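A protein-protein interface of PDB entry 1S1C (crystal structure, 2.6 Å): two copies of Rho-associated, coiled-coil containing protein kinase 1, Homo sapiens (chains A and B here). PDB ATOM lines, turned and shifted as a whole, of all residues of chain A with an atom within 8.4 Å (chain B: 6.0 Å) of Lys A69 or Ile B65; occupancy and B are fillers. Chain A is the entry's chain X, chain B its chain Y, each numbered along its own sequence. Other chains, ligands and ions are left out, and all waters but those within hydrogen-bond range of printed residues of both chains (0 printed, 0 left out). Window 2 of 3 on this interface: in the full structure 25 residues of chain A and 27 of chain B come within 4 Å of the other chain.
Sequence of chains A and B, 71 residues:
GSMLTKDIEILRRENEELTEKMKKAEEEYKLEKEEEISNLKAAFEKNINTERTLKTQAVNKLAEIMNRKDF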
ATOM      1  N   LEU A  62      32.691   0.122 -23.687  1.00  0.00           N
ATOM      2  CA  LEU A  62      31.425  -0.576 -23.528  1.00  0.00           C
ATOM      3  C   LEU A  62      30.949  -0.371 -22.096  1.00  0.00           C
ATOM      4  O   LEU A  62      29.761  -0.137 -21.842  1.00  0.00           O
ATOM      5  CB  LEU A  62      31.609  -2.065 -23.795  1.00  0.00           C
ATOM      6  CG  LEU A  62      30.569  -2.717 -24.703  1.00  0.00           C
ATOM      7  CD1 LEU A  62      30.789  -4.222 -24.693  1.00  0.00           C
ATOM      8  CD2 LEU A  62      29.158  -2.376 -24.233  1.00  0.00           C
ATOM      9  N   ALA A  63      31.884  -0.459 -21.157  1.00  0.00           N
ATOM     10  CA  ALA A  63      31.558  -0.274 -19.747  1.00  0.00           C
ATOM     11  C   ALA A  63      31.080   1.158 -19.550  1.00  0.00           C
ATOM     12  O   ALA A  63      30.043   1.396 -18.939  1.00  0.00           O
ATOM     13  CB  ALA A  63      32.783  -0.565 -18.876  1.00  0.00           C
ATOM     14  N   GLU A  64      31.806   2.113 -20.124  1.00  0.00           N
ATOM     15  CA  GLU A  64      31.421   3.512 -20.003  1.00  0.00           C
ATOM     16  C   GLU A  64      30.012   3.709 -20.546  1.00  0.00           C
ATOM     17  O   GLU A  64      29.182   4.358 -19.917  1.00  0.00           O
ATOM     18  CB  GLU A  64      32.383   4.418 -20.779  1.00  0.00           C
ATOM     19  CG  GLU A  64      32.022   5.908 -20.691  1.00  0.00           C
ATOM     20  CD  GLU A  64      32.708   6.772 -21.751  1.00  0.00           C
ATOM     21  OE1 GLU A  64      32.453   6.564 -22.947  1.00  0.00           O
ATOM     22  OE2 GLU A  64      33.504   7.666 -21.399  1.00  0.00           O
ATOM     23  N   ILE A  65      29.737   3.130 -21.711  1.00  0.00           N
ATOM     24  CA  ILE A  65      28.438   3.291 -22.354  1.00  0.00           C
ATOM     25  C   ILE A  65      27.266   2.678 -21.593  1.00  0.00           C
ATOM     26  O   ILE A  65      26.218   3.302 -21.459  1.00  0.00           O
ATOM     27  CB  ILE A  65      28.465   2.713 -23.782  1.00  0.00           C
ATOM     28  CG1 ILE A  65      29.500   3.459 -24.622  1.00  0.00           C
ATOM     29  CG2 ILE A  65      27.098   2.826 -24.418  1.00  0.00           C
ATOM     30  CD1 ILE A  65      29.205   4.938 -24.789  1.00  0.00           C
ATOM     31  N   MET A  66      27.447   1.457 -21.097  1.00  0.00           N
ATOM     32  CA  MET A  66      26.396   0.763 -20.356  1.00  0.00           C
ATOM     33  C   MET A  66      26.163   1.355 -18.975  1.00  0.00           C
ATOM     34  O   MET A  66      25.048   1.341 -18.459  1.00  0.00           O
ATOM     35  CB  MET A  66      26.727  -0.723 -20.229  1.00  0.00           C
ATOM     36  CG  MET A  66      26.781  -1.487 -21.542  1.00  0.00           C
ATOM     37  SD  MET A  66      25.211  -1.480 -22.435  1.00  0.00           S
ATOM     38  CE  MET A  66      24.190  -2.485 -21.353  1.00  0.00           C
ATOM     39  N   ASN A  67      27.200   1.919 -18.386  1.00  0.00           N
ATOM     40  CA  ASN A  67      26.990   2.524 -17.094  1.00  0.00           C
ATOM     41  C   ASN A  67      26.152   3.787 -17.302  1.00  0.00           C
ATOM     42  O   ASN A  67      25.604   4.348 -16.358  1.00  0.00           O
ATOM     43  CB  ASN A  67      28.317   2.873 -16.440  1.00  0.00           C
ATOM     44  CG  ASN A  67      28.219   2.865 -14.945  1.00  0.00           C
ATOM     45  OD1 ASN A  67      27.919   1.832 -14.342  1.00  0.00           O
ATOM     46  ND2 ASN A  67      28.445   4.014 -14.330  1.00  0.00           N
ATOM     47  N   ARG A  68      26.049   4.217 -18.555  1.00  0.00           N
ATOM     48  CA  ARG A  68      25.280   5.406 -18.908  1.00  0.00           C
ATOM     49  C   ARG A  68      23.933   5.064 -19.545  1.00  0.00           C
ATOM     50  O   ARG A  68      23.133   5.957 -19.794  1.00  0.00           O
ATOM     51  CB  ARG A  68      26.065   6.285 -19.886  1.00  0.00           C
ATOM     52  CG  ARG A  68      26.700   7.532 -19.294  1.00  0.00           C
ATOM     53  CD  ARG A  68      28.164   7.322 -18.963  1.00  0.00           C
ATOM     54  NE  ARG A  68      28.355   6.549 -17.741  1.00  0.00           N
ATOM     55  CZ  ARG A  68      29.537   6.127 -17.299  1.00  0.00           C
ATOM     56  NH1 ARG A  68      30.644   6.398 -17.980  1.00  0.00           N
ATOM     57  NH2 ARG A  68      29.614   5.432 -16.171  1.00  0.00           N
ATOM     58  N   LYS A  69      23.694   3.782 -19.822  1.00  0.00           N
ATOM     59  CA  LYS A  69      22.434   3.342 -20.435  1.00  0.00           C
ATOM     60  C   LYS A  69      21.277   3.260 -19.438  1.00  0.00           C
ATOM     61  O   LYS A  69      20.259   3.951 -19.671  1.00  0.00           O
ATOM     62  CB  LYS A  69      22.602   1.975 -21.106  1.00  0.00           C
ATOM     63  CG  LYS A  69      23.358   2.005 -22.417  1.00  0.00           C
ATOM     64  CD  LYS A  69      22.623   2.815 -23.470  1.00  0.00           C
ATOM     65  CE  LYS A  69      23.354   2.767 -24.803  1.00  0.00           C
ATOM     66  NZ  LYS A  69      22.649   3.555 -25.847  1.00  0.00           N
ATOM     67  N   ASN B  60      31.559  -5.609 -31.631  1.00  0.00           N
ATOM     68  CA  ASN B  60      30.227  -5.894 -32.165  1.00  0.00           C
ATOM     69  C   ASN B  60      29.119  -5.589 -31.156  1.00  0.00           C
ATOM     70  O   ASN B  60      28.040  -5.120 -31.532  1.00  0.00           O
ATOM     71  CB  ASN B  60      30.108  -7.362 -32.616  1.00  0.00           C
ATOM     72  CG  ASN B  60      31.039  -7.708 -33.784  1.00  0.00           C
ATOM     73  OD1 ASN B  60      31.540  -6.830 -34.479  1.00  0.00           O
ATOM     74  ND2 ASN B  60      31.257  -9.003 -34.004  1.00  0.00           N
ATOM     75  N   LYS B  61      29.381  -5.851 -29.877  1.00  0.00           N
ATOM     76  CA  LYS B  61      28.390  -5.596 -28.842  1.00  0.00           C
ATOM     77  C   LYS B  61      28.192  -4.089 -28.683  1.00  0.00           C
ATOM     78  O   LYS B  61      27.082  -3.615 -28.438  1.00  0.00           O
ATOM     79  CB  LYS B  61      28.849  -6.196 -27.515  1.00  0.00           C
ATOM     80  CG  LYS B  61      27.789  -6.160 -26.430  1.00  0.00           C
ATOM     81  CD  LYS B  61      26.624  -7.064 -26.805  1.00  0.00           C
ATOM     82  CE  LYS B  61      25.515  -7.033 -25.769  1.00  0.00           C
ATOM     83  NZ  LYS B  61      24.410  -7.971 -26.145  1.00  0.00           N
ATOM     84  N   LEU B  62      29.281  -3.339 -28.818  1.00  0.00           N
ATOM     85  CA  LEU B  62      29.232  -1.891 -28.701  1.00  0.00           C
ATOM     86  C   LEU B  62      28.358  -1.359 -29.826  1.00  0.00           C
ATOM     87  O   LEU B  62      27.547  -0.449 -29.628  1.00  0.00           O
ATOM     88  CB  LEU B  62      30.635  -1.302 -28.825  1.00  0.00           C
ATOM     89  CG  LEU B  62      31.017  -0.250 -27.791  1.00  0.00           C
ATOM     90  CD1 LEU B  62      32.342   0.359 -28.180  1.00  0.00           C
ATOM     91  CD2 LEU B  62      29.934   0.817 -27.696  1.00  0.00           C
ATOM     92  N   ALA B  63      28.532  -1.935 -31.010  1.00  0.00           N
ATOM     93  CA  ALA B  63      27.752  -1.529 -32.168  1.00  0.00           C
ATOM     94  C   ALA B  63      26.282  -1.860 -31.943  1.00  0.00           C
ATOM     95  O   ALA B  63      25.416  -0.993 -32.059  1.00  0.00           O
ATOM     96  CB  ALA B  63      28.260  -2.240 -33.425  1.00  0.00           C
ATOM     97  N   GLU B  64      26.012  -3.132 -31.662  1.00  0.00           N
ATOM     98  CA  GLU B  64      24.656  -3.612 -31.427  1.00  0.00           C
ATOM     99  C   GLU B  64      23.899  -2.691 -30.478  1.00  0.00           C
ATOM    100  O   GLU B  64      22.771  -2.284 -30.753  1.00  0.00           O
ATOM    101  CB  GLU B  64      24.700  -5.025 -30.844  1.00  0.00           C
ATOM    102  CG  GLU B  64      23.495  -5.383 -29.964  1.00  0.00           C
ATOM    103  CD  GLU B  64      23.535  -6.820 -29.476  1.00  0.00           C
ATOM    104  OE1 GLU B  64      24.271  -7.631 -30.091  1.00  0.00           O
ATOM    105  OE2 GLU B  64      22.822  -7.145 -28.496  1.00  0.00           O
ATOM    106  N   ILE B  65      24.519  -2.383 -29.351  1.00  0.00           N
ATOM    107  CA  ILE B  65      23.906  -1.510 -28.367  1.00  0.00           C
ATOM    108  C   ILE B  65      23.720  -0.071 -28.858  1.00  0.00           C
ATOM    109  O   ILE B  65      22.680   0.537 -28.633  1.00  0.00           O
ATOM    110  CB  ILE B  65      24.741  -1.492 -27.073  1.00  0.00           C
ATOM    111  CG1 ILE B  65      24.764  -2.890 -26.455  1.00  0.00           C
ATOM    112  CG2 ILE B  65      24.157  -0.498 -26.094  1.00  0.00           C
ATOM    113  CD1 ILE B  65      23.394  -3.412 -26.061  1.00  0.00           C
ATOM    114  N   MET B  66      24.734   0.470 -29.523  1.00  0.00           N
ATOM    115  CA  MET B  66      24.675   1.836 -30.021  1.00  0.00           C
ATOM    116  C   MET B  66      23.811   2.008 -31.278  1.00  0.00           C
ATOM    117  O   MET B  66      23.140   3.026 -31.435  1.00  0.00           O
ATOM    118  CB  MET B  66      26.085   2.337 -30.357  1.00  0.00           C
ATOM    119  CG  MET B  66      27.063   2.431 -29.197  1.00  0.00           C
ATOM    120  SD  MET B  66      26.547   3.589 -27.922  1.00  0.00           S
ATOM    121  CE  MET B  66      26.705   5.169 -28.813  1.00  0.00           C
ATOM    122  N   ASN B  67      23.856   1.029 -32.185  1.00  0.00           N
ATOM    123  CA  ASN B  67      23.175   1.104 -33.491  1.00  0.00           C
ATOM    124  C   ASN B  67      21.656   1.122 -33.559  1.00  0.00           C
ATOM    125  O   ASN B  67      20.978   0.235 -33.048  1.00  0.00           O
ATOM    126  CB  ASN B  67      23.701  -0.005 -34.406  1.00  0.00           C
ATOM    127  CG  ASN B  67      23.443   0.275 -35.883  1.00  0.00           C
ATOM    128  OD1 ASN B  67      23.679  -0.583 -36.736  1.00  0.00           O
ATOM    129  ND2 ASN B  67      22.964   1.478 -36.190  1.00  0.00           N
ATOM    130  N   ASP B  70      19.404  -1.375 -36.249  1.00  0.00           N
ATOM    131  CA  ASP B  70      19.468  -2.780 -35.882  1.00  0.00           C
ATOM    132  C   ASP B  70      18.445  -3.068 -34.786  1.00  0.00           C
ATOM    133  O   ASP B  70      18.848  -3.255 -33.618  1.00  0.00           O
ATOM    134  CB  ASP B  70      20.886  -3.124 -35.411  1.00  0.00           C
ATOM    135  CG  ASP B  70      20.993  -4.523 -34.837  1.00  0.00           C
ATOM    136  OD1 ASP B  70      20.627  -5.492 -35.535  1.00  0.00           O
ATOM    137  OD2 ASP B  70      21.445  -4.648 -33.681  1.00  0.00           O
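Leu B62 touches its own counterpart, Leu A62. Ile A65 touches Met B66, and with the chains exchanged Met A66 touches Ile B65. Positions printed for both chains: 62, 63, 64, 65, 66 and 67.
Hydrophobic or aromatic side chains of chain A within 4 Å of the printed part of chain B: Leu A62, Ile A65 and Met A66. Hydrophobic or aromatic side chains of chain B within 4 Å of the printed part of chain A: Leu B62, Ile B65 and Met B66. Among the printed residues, 5 pairs touch across the chains. Among the printed residues, no Asp or Glu carboxylate lies within 4 Å of a Lys or Arg side-chain nitrogen of the other chain.
Printed residues of chain B within 4 Å of Lys A69: Ile B65. Of the printed residues of chain A, Ile B65 touches Met A66 and Lys A69. Of the printed residues of chain B, Leu A62 touches Lys B61 and Leu B62. Printed residues of chain A within 4 Å of Lys B61: Leu A62. Of the printed residues of chain A, Met B66 touches Ile A65. Printed residues of chain B within 4 Å of Ile A65: Met B66 (3.6 Å). The nearest residue of chain B that does not touch Lys A69 is Met B66 (4.4 Å). The nearest residue of chain A that does not touch Ile B65 is Ile A65 (4.7 Å).
Leu A62 touches Lys B61 (CD1 to CB, 3.95 Å). Leu B62 touches Leu A62. CG2 of Ile A65 touches SD of Met B66, 3.6 Å away. Ile B65 touches Met A66 (CG2 to SD, 3.9 Å). CE of Lys A69 touches CG2 of Ile B65 (3.6 Å).
The side-chain carboxylate (OE2) of Glu B64 lies within salt-bridge range of the side-chain amino group (NZ) of Lys B61, at 3.0 Å.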
